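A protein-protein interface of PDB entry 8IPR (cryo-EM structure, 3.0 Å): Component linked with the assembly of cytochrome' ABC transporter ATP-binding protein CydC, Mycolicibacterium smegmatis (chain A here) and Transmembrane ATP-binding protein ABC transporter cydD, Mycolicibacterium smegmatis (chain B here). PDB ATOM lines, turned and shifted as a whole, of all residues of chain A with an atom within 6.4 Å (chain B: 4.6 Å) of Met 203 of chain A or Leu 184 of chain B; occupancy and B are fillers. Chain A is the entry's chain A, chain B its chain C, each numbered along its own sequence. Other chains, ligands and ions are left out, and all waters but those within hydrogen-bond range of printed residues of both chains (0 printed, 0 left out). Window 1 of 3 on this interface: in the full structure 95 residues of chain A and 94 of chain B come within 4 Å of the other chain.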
ATOM      1  N   SER A 115     -15.353  21.647   5.396  1.00  0.00           N
ATOM      2  CA  SER A 115     -14.370  20.616   5.722  1.00  0.00           C
ATOM      3  C   SER A 115     -12.950  21.161   5.663  1.00  0.00           C
ATOM      4  O   SER A 115     -12.105  20.795   6.488  1.00  0.00           O
ATOM      5  CB  SER A 115     -14.526  19.426   4.777  1.00  0.00           C
ATOM      6  OG  SER A 115     -15.755  18.759   4.996  1.00  0.00           O
ATOM      7  N   GLY A 116     -12.662  22.026   4.687  1.00  0.00           N
ATOM      8  CA  GLY A 116     -11.322  22.577   4.575  1.00  0.00           C
ATOM      9  C   GLY A 116     -10.939  23.431   5.769  1.00  0.00           C
ATOM     10  O   GLY A 116      -9.812  23.353   6.263  1.00  0.00           O
ATOM     11  N   LEU A 118     -12.198  23.062   8.766  1.00  0.00           N
ATOM     12  CA  LEU A 118     -12.015  22.126   9.869  1.00  0.00           C
ATOM     13  C   LEU A 118     -10.627  21.503   9.834  1.00  0.00           C
ATOM     14  O   LEU A 118      -9.963  21.395  10.869  1.00  0.00           O
ATOM     15  CB  LEU A 118     -13.092  21.044   9.819  1.00  0.00           C
ATOM     16  CG  LEU A 118     -14.468  21.446  10.348  1.00  0.00           C
ATOM     17  CD1 LEU A 118     -15.472  20.340  10.097  1.00  0.00           C
ATOM     18  CD2 LEU A 118     -14.389  21.775  11.826  1.00  0.00           C
ATOM     19  N   VAL A 119     -10.169  21.100   8.647  1.00  0.00           N
ATOM     20  CA  VAL A 119      -8.830  20.528   8.517  1.00  0.00           C
ATOM     21  C   VAL A 119      -7.775  21.550   8.922  1.00  0.00           C
ATOM     22  O   VAL A 119      -6.874  21.263   9.723  1.00  0.00           O
ATOM     23  CB  VAL A 119      -8.604  20.028   7.078  1.00  0.00           C
ATOM     24  CG1 VAL A 119      -7.123  19.823   6.810  1.00  0.00           C
ATOM     25  CG2 VAL A 119      -9.379  18.751   6.829  1.00  0.00           C
ATOM     26  N   LEU A 122      -7.910  22.168  12.775  1.00  0.00           N
ATOM     27  CA  LEU A 122      -7.593  21.039  13.636  1.00  0.00           C
ATOM     28  C   LEU A 122      -6.218  20.455  13.358  1.00  0.00           C
ATOM     29  O   LEU A 122      -5.796  19.536  14.065  1.00  0.00           O
ATOM     30  CB  LEU A 122      -8.661  19.954  13.493  1.00  0.00           C
ATOM     31  CG  LEU A 122     -10.013  20.331  14.100  1.00  0.00           C
ATOM     32  CD1 LEU A 122     -11.128  19.597  13.392  1.00  0.00           C
ATOM     33  CD2 LEU A 122     -10.037  20.042  15.592  1.00  0.00           C
ATOM     34  N   ARG A 198      -7.217  27.900   0.876  1.00  0.00           N
ATOM     35  CA  ARG A 198      -6.623  27.015  -0.116  1.00  0.00           C
ATOM     36  C   ARG A 198      -7.227  25.621  -0.048  1.00  0.00           C
ATOM     37  O   ARG A 198      -7.534  25.024  -1.082  1.00  0.00           O
ATOM     38  CB  ARG A 198      -5.110  26.957   0.090  1.00  0.00           C
ATOM     39  CG  ARG A 198      -4.377  26.065  -0.883  1.00  0.00           C
ATOM     40  CD  ARG A 198      -3.079  25.573  -0.277  1.00  0.00           C
ATOM     41  NE  ARG A 198      -3.317  24.653   0.826  1.00  0.00           N
ATOM     42  CZ  ARG A 198      -2.380  24.209   1.650  1.00  0.00           C
ATOM     43  NH1 ARG A 198      -1.116  24.579   1.522  1.00  0.00           N
ATOM     44  NH2 ARG A 198      -2.717  23.373   2.627  1.00  0.00           N
ATOM     45  N   ASP A 199      -7.413  25.083   1.157  1.00  0.00           N
ATOM     46  CA  ASP A 199      -7.901  23.716   1.288  1.00  0.00           C
ATOM     47  C   ASP A 199      -9.419  23.621   1.339  1.00  0.00           C
ATOM     48  O   ASP A 199      -9.955  22.522   1.175  1.00  0.00           O
ATOM     49  CB  ASP A 199      -7.312  23.050   2.534  1.00  0.00           C
ATOM     50  CG  ASP A 199      -7.177  24.005   3.690  1.00  0.00           C
ATOM     51  OD1 ASP A 199      -7.740  25.112   3.601  1.00  0.00           O
ATOM     52  OD2 ASP A 199      -6.503  23.653   4.681  1.00  0.00           O
ATOM     53  N   THR A 200     -10.126  24.730   1.562  1.00  0.00           N
ATOM     54  CA  THR A 200     -11.578  24.708   1.417  1.00  0.00           C
ATOM     55  C   THR A 200     -11.962  24.383  -0.020  1.00  0.00           C
ATOM     56  O   THR A 200     -12.737  23.453  -0.278  1.00  0.00           O
ATOM     57  CB  THR A 200     -12.170  26.051   1.844  1.00  0.00           C
ATOM     58  OG1 THR A 200     -11.813  26.322   3.204  1.00  0.00           O
ATOM     59  CG2 THR A 200     -13.680  26.026   1.727  1.00  0.00           C
ATOM     60  N   ALA A 201     -11.402  25.127  -0.971  1.00  0.00           N
ATOM     61  CA  ALA A 201     -11.509  24.812  -2.392  1.00  0.00           C
ATOM     62  C   ALA A 201     -10.321  23.924  -2.732  1.00  0.00           C
ATOM     63  O   ALA A 201      -9.236  24.397  -3.065  1.00  0.00           O
ATOM     64  CB  ALA A 201     -11.533  26.081  -3.233  1.00  0.00           C
ATOM     65  N   GLY A 202     -10.545  22.618  -2.676  1.00  0.00           N
ATOM     66  CA  GLY A 202      -9.479  21.639  -2.718  1.00  0.00           C
ATOM     67  C   GLY A 202      -9.853  20.450  -1.863  1.00  0.00           C
ATOM     68  O   GLY A 202      -9.326  19.349  -2.035  1.00  0.00           O
ATOM     69  N   MET A 203     -10.774  20.675  -0.927  1.00  0.00           N
ATOM     70  CA  MET A 203     -11.621  19.615  -0.402  1.00  0.00           C
ATOM     71  C   MET A 203     -13.009  19.643  -1.014  1.00  0.00           C
ATOM     72  O   MET A 203     -13.626  18.586  -1.176  1.00  0.00           O
ATOM     73  CB  MET A 203     -11.736  19.705   1.124  1.00  0.00           C
ATOM     74  CG  MET A 203     -10.419  19.546   1.861  1.00  0.00           C
ATOM     75  SD  MET A 203     -10.170  17.878   2.491  1.00  0.00           S
ATOM     76  CE  MET A 203     -11.802  17.510   3.122  1.00  0.00           C
ATOM     77  N   LEU A 204     -13.505  20.830  -1.375  1.00  0.00           N
ATOM     78  CA  LEU A 204     -14.708  20.905  -2.198  1.00  0.00           C
ATOM     79  C   LEU A 204     -14.521  20.147  -3.504  1.00  0.00           C
ATOM     80  O   LEU A 204     -15.444  19.480  -3.985  1.00  0.00           O
ATOM     81  CB  LEU A 204     -15.062  22.365  -2.472  1.00  0.00           C
ATOM     82  CG  LEU A 204     -16.097  22.620  -3.568  1.00  0.00           C
ATOM     83  CD1 LEU A 204     -17.475  22.200  -3.105  1.00  0.00           C
ATOM     84  CD2 LEU A 204     -16.088  24.078  -3.984  1.00  0.00           C
ATOM     85  N   ALA A 205     -13.326  20.236  -4.093  1.00  0.00           N
ATOM     86  CA  ALA A 205     -13.050  19.509  -5.325  1.00  0.00           C
ATOM     87  C   ALA A 205     -12.973  18.007  -5.091  1.00  0.00           C
ATOM     88  O   ALA A 205     -13.226  17.227  -6.015  1.00  0.00           O
ATOM     89  CB  ALA A 205     -11.750  20.013  -5.951  1.00  0.00           C
ATOM     90  N   LEU A 206     -12.621  17.582  -3.880  1.00  0.00           N
ATOM     91  CA  LEU A 206     -12.457  16.162  -3.601  1.00  0.00           C
ATOM     92  C   LEU A 206     -13.769  15.476  -3.244  1.00  0.00           C
ATOM     93  O   LEU A 206     -14.032  14.368  -3.723  1.00  0.00           O
ATOM     94  CB  LEU A 206     -11.442  15.957  -2.474  1.00  0.00           C
ATOM     95  CG  LEU A 206      -9.967  16.065  -2.865  1.00  0.00           C
ATOM     96  CD1 LEU A 206      -9.087  16.047  -1.633  1.00  0.00           C
ATOM     97  CD2 LEU A 206      -9.576  14.948  -3.815  1.00  0.00           C
ATOM     98  N   GLU A 207     -14.602  16.102  -2.412  1.00  0.00           N
ATOM     99  CA  GLU A 207     -15.855  15.456  -2.029  1.00  0.00           C
ATOM    100  C   GLU A 207     -16.906  15.508  -3.131  1.00  0.00           C
ATOM    101  O   GLU A 207     -17.696  14.569  -3.266  1.00  0.00           O
ATOM    102  CB  GLU A 207     -16.415  16.078  -0.749  1.00  0.00           C
ATOM    103  CG  GLU A 207     -15.578  15.826   0.486  1.00  0.00           C
ATOM    104  CD  GLU A 207     -16.127  16.517   1.715  1.00  0.00           C
ATOM    105  OE1 GLU A 207     -17.049  17.345   1.568  1.00  0.00           O
ATOM    106  OE2 GLU A 207     -15.636  16.232   2.827  1.00  0.00           O
ATOM    107  N   HIS A 208     -16.939  16.576  -3.922  1.00  0.00           N
ATOM    108  CA  HIS A 208     -17.978  16.777  -4.925  1.00  0.00           C
ATOM    109  C   HIS A 208     -17.384  16.891  -6.322  1.00  0.00           C
ATOM    110  O   HIS A 208     -17.773  17.750  -7.114  1.00  0.00           O
ATOM    111  CB  HIS A 208     -18.816  18.006  -4.591  1.00  0.00           C
ATOM    112  CG  HIS A 208     -19.470  17.938  -3.246  1.00  0.00           C
ATOM    113  ND1 HIS A 208     -19.057  18.702  -2.178  1.00  0.00           N
ATOM    114  CD2 HIS A 208     -20.504  17.189  -2.795  1.00  0.00           C
ATOM    115  CE1 HIS A 208     -19.809  18.431  -1.127  1.00  0.00           C
ATOM    116  NE2 HIS A 208     -20.696  17.517  -1.475  1.00  0.00           N
ATOM    117  N   VAL A 221     -12.247  25.669  -9.292  1.00  0.00           N
ATOM    118  CA  VAL A 221     -11.877  25.303  -7.927  1.00  0.00           C
ATOM    119  C   VAL A 221     -10.377  25.049  -7.831  1.00  0.00           C
ATOM    120  O   VAL A 221      -9.714  25.491  -6.881  1.00  0.00           O
ATOM    121  CB  VAL A 221     -12.693  24.083  -7.462  1.00  0.00           C
ATOM    122  CG1 VAL A 221     -12.253  23.648  -6.080  1.00  0.00           C
ATOM    123  CG2 VAL A 221     -14.171  24.411  -7.462  1.00  0.00           C
ATOM    124  N   PHE A 225      -7.515  27.060  -5.702  1.00  0.00           N
ATOM    125  CA  PHE A 225      -6.526  26.359  -4.889  1.00  0.00           C
ATOM    126  C   PHE A 225      -5.119  26.882  -5.169  1.00  0.00           C
ATOM    127  O   PHE A 225      -4.381  27.246  -4.244  1.00  0.00           O
ATOM    128  CB  PHE A 225      -6.614  24.855  -5.159  1.00  0.00           C
ATOM    129  CG  PHE A 225      -5.656  24.026  -4.350  1.00  0.00           C
ATOM    130  CD1 PHE A 225      -4.374  23.772  -4.808  1.00  0.00           C
ATOM    131  CD2 PHE A 225      -6.044  23.483  -3.141  1.00  0.00           C
ATOM    132  CE1 PHE A 225      -3.498  23.011  -4.068  1.00  0.00           C
ATOM    133  CE2 PHE A 225      -5.171  22.720  -2.395  1.00  0.00           C
ATOM    134  CZ  PHE A 225      -3.897  22.483  -2.860  1.00  0.00           C
ATOM    135  N   HIS A 377     -26.141  10.168   9.255  1.00  0.00           N
ATOM    136  CA  HIS A 377     -24.831   9.901   8.683  1.00  0.00           C
ATOM    137  C   HIS A 377     -24.577   8.407   8.540  1.00  0.00           C
ATOM    138  O   HIS A 377     -24.884   7.621   9.439  1.00  0.00           O
ATOM    139  CB  HIS A 377     -23.734  10.525   9.544  1.00  0.00           C
ATOM    140  CG  HIS A 377     -22.429  10.685   8.833  1.00  0.00           C
ATOM    141  ND1 HIS A 377     -22.317  11.340   7.626  1.00  0.00           N
ATOM    142  CD2 HIS A 377     -21.180  10.277   9.156  1.00  0.00           C
ATOM    143  CE1 HIS A 377     -21.056  11.327   7.236  1.00  0.00           C
ATOM    144  NE2 HIS A 377     -20.345  10.688   8.146  1.00  0.00           N
ATOM    145  N   ALA B 101      -6.408  13.816   0.180  1.00  0.00           N
ATOM    146  CA  ALA B 101      -6.657  15.008   0.981  1.00  0.00           C
ATOM    147  C   ALA B 101      -5.540  15.238   1.987  1.00  0.00           C
ATOM    148  O   ALA B 101      -5.093  16.373   2.180  1.00  0.00           O
ATOM    149  CB  ALA B 101      -8.002  14.889   1.694  1.00  0.00           C
ATOM    150  N   GLN B 180      -6.657  11.961  10.442  1.00  0.00           N
ATOM    151  CA  GLN B 180      -7.387  13.079   9.849  1.00  0.00           C
ATOM    152  C   GLN B 180      -8.711  12.617   9.254  1.00  0.00           C
ATOM    153  O   GLN B 180      -9.754  13.251   9.461  1.00  0.00           O
ATOM    154  CB  GLN B 180      -6.533  13.768   8.784  1.00  0.00           C
ATOM    155  CG  GLN B 180      -7.294  14.817   7.989  1.00  0.00           C
ATOM    156  CD  GLN B 180      -6.406  15.608   7.053  1.00  0.00           C
ATOM    157  OE1 GLN B 180      -5.477  16.287   7.488  1.00  0.00           O
ATOM    158  NE2 GLN B 180      -6.692  15.531   5.762  1.00  0.00           N
ATOM    159  N   GLY B 181      -8.691  11.502   8.518  1.00  0.00           N
ATOM    160  CA  GLY B 181      -9.919  11.014   7.913  1.00  0.00           C
ATOM    161  C   GLY B 181     -10.967  10.634   8.940  1.00  0.00           C
ATOM    162  O   GLY B 181     -12.143  10.989   8.803  1.00  0.00           O
ATOM    163  N   ARG B 182     -10.559   9.916   9.989  1.00  0.00           N
ATOM    164  CA  ARG B 182     -11.523   9.503  11.001  1.00  0.00           C
ATOM    165  C   ARG B 182     -12.063  10.696  11.776  1.00  0.00           C
ATOM    166  O   ARG B 182     -13.251  10.729  12.117  1.00  0.00           O
ATOM    167  CB  ARG B 182     -10.896   8.482  11.947  1.00  0.00           C
ATOM    168  CG  ARG B 182     -10.578   7.158  11.275  1.00  0.00           C
ATOM    169  CD  ARG B 182     -10.002   6.158  12.264  1.00  0.00           C
ATOM    170  NE  ARG B 182      -9.629   4.908  11.612  1.00  0.00           N
ATOM    171  CZ  ARG B 182      -9.000   3.907  12.215  1.00  0.00           C
ATOM    172  NH1 ARG B 182      -8.670   3.969  13.494  1.00  0.00           N
ATOM    173  NH2 ARG B 182      -8.696   2.818  11.517  1.00  0.00           N
ATOM    174  N   MET B 183     -11.217  11.690  12.063  1.00  0.00           N
ATOM    175  CA  MET B 183     -11.700  12.881  12.755  1.00  0.00           C
ATOM    176  C   MET B 183     -12.714  13.638  11.906  1.00  0.00           C
ATOM    177  O   MET B 183     -13.752  14.082  12.415  1.00  0.00           O
ATOM    178  CB  MET B 183     -10.527  13.784  13.130  1.00  0.00           C
ATOM    179  CG  MET B 183     -10.931  15.190  13.539  1.00  0.00           C
ATOM    180  SD  MET B 183     -10.803  15.472  15.315  1.00  0.00           S
ATOM    181  CE  MET B 183      -9.075  15.101  15.589  1.00  0.00           C
ATOM    182  N   LEU B 184     -12.437  13.788  10.608  1.00  0.00           N
ATOM    183  CA  LEU B 184     -13.390  14.457   9.727  1.00  0.00           C
ATOM    184  C   LEU B 184     -14.709  13.698   9.664  1.00  0.00           C
ATOM    185  O   LEU B 184     -15.788  14.304   9.724  1.00  0.00           O
ATOM    186  CB  LEU B 184     -12.799  14.608   8.327  1.00  0.00           C
ATOM    187  CG  LEU B 184     -11.897  15.811   8.054  1.00  0.00           C
ATOM    188  CD1 LEU B 184     -11.767  16.020   6.558  1.00  0.00           C
ATOM    189  CD2 LEU B 184     -12.432  17.061   8.729  1.00  0.00           C
ATOM    190  N   ASP B 185     -14.645  12.369   9.547  1.00  0.00           N
ATOM    191  CA  ASP B 185     -15.868  11.574   9.488  1.00  0.00           C
ATOM    192  C   ASP B 185     -16.664  11.684  10.782  1.00  0.00           C
ATOM    193  O   ASP B 185     -17.896  11.785  10.755  1.00  0.00           O
ATOM    194  CB  ASP B 185     -15.530  10.114   9.193  1.00  0.00           C
ATOM    195  CG  ASP B 185     -16.734   9.322   8.727  1.00  0.00           C
ATOM    196  OD1 ASP B 185     -17.827   9.910   8.602  1.00  0.00           O
ATOM    197  OD2 ASP B 185     -16.589   8.106   8.490  1.00  0.00           O
ATOM    198  N   LEU B 186     -15.981  11.659  11.928  1.00  0.00           N
ATOM    199  CA  LEU B 186     -16.676  11.760  13.205  1.00  0.00           C
ATOM    200  C   LEU B 186     -17.326  13.127  13.379  1.00  0.00           C
ATOM    201  O   LEU B 186     -18.432  13.226  13.922  1.00  0.00           O
ATOM    202  CB  LEU B 186     -15.709  11.479  14.352  1.00  0.00           C
ATOM    203  CG  LEU B 186     -15.572  10.011  14.748  1.00  0.00           C
ATOM    204  CD1 LEU B 186     -14.634   9.876  15.925  1.00  0.00           C
ATOM    205  CD2 LEU B 186     -16.930   9.421  15.074  1.00  0.00           C
ATOM    206  N   ILE B 187     -16.653  14.192  12.942  1.00  0.00           N
ATOM    207  CA  ILE B 187     -17.255  15.519  13.028  1.00  0.00           C
ATOM    208  C   ILE B 187     -18.454  15.624  12.095  1.00  0.00           C
ATOM    209  O   ILE B 187     -19.451  16.282  12.415  1.00  0.00           O
ATOM    210  CB  ILE B 187     -16.202  16.603  12.740  1.00  0.00           C
ATOM    211  CG1 ILE B 187     -15.131  16.590  13.826  1.00  0.00           C
ATOM    212  CG2 ILE B 187     -16.845  17.977  12.668  1.00  0.00           C
ATOM    213  CD1 ILE B 187     -14.024  17.570  13.587  1.00  0.00           C
ATOM    214  N   ALA B 188     -18.386  14.971  10.932  1.00  0.00           N
ATOM    215  CA  ALA B 188     -19.508  15.012   9.999  1.00  0.00           C
ATOM    216  C   ALA B 188     -20.751  14.342  10.570  1.00  0.00           C
ATOM    217  O   ALA B 188     -21.871  14.661  10.154  1.00  0.00           O
ATOM    218  CB  ALA B 188     -19.116  14.355   8.676  1.00  0.00           C
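Hydrophobic or aromatic side chains of chain A that line the printed part of chain B: Leu 118, Val 119, Leu 122, Met 203, Leu 206 and His 377.
Of the 10 printed residues of chain B, 6 touch a printed residue of chain A.
Among the printed residues, 9 pairs touch across the chains.
Among the printed residues, no Asp or Glu carboxylate lies within 4 Å of a Lys or Arg side-chain nitrogen of the other chain.
Printed residues of chain B within 4 Å of Met 203 of chain A: Ala 101 (3.8 Å) and Leu 184 (3.7 Å).
Printed residues of chain A within 4 Å of Gln 180 of chain B: Val 119.
Of the printed residues of chain B, Val 119 of chain A touches Gln 180 (3.96 Å) and Leu 184 (3.6 Å).
Printed residues of chain A within 4 Å of Ala 101 of chain B: Met 203 (3.8 Å) and Leu 206 (3.7 Å).
Of the printed residues of chain A, Asp 185 of chain B touches His 377 (2.7 Å).
His 208 of chain A touches none of the printed residues of chain B.
The nearest residue of chain A that does not touch Leu 184 of chain B is Leu 118 of chain A (4.2 Å).
The nearest printed residue of chain A that does not touch Gln 180 of chain B is Met 203 of chain A (5.3 Å).
NE2 of His 377 of chain A sits at hydrogen-bond distance from OD1 of Asp 185 of chain B (2.7 Å).
Among the printed residues, merely in contact across the chains: Leu 118 of chain A with Ile 187 of chain B (3.8 Å), Val 119 of chain A with Gln 180 of chain B (3.96 Å), Val 119 of chain A with Leu 184 of chain B (3.6 Å), Leu 122 of chain A with Ile 187 of chain B (3.5 Å), Met 203 of chain A with Ala 101 of chain B (3.8 Å), Met 203 of chain A with Leu 184 of chain B (3.7 Å), Leu 206 of chain A with Ala 101 of chain B (3.7 Å) and His 377 of chain A with Ala 188 of chain B (3.9 Å).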
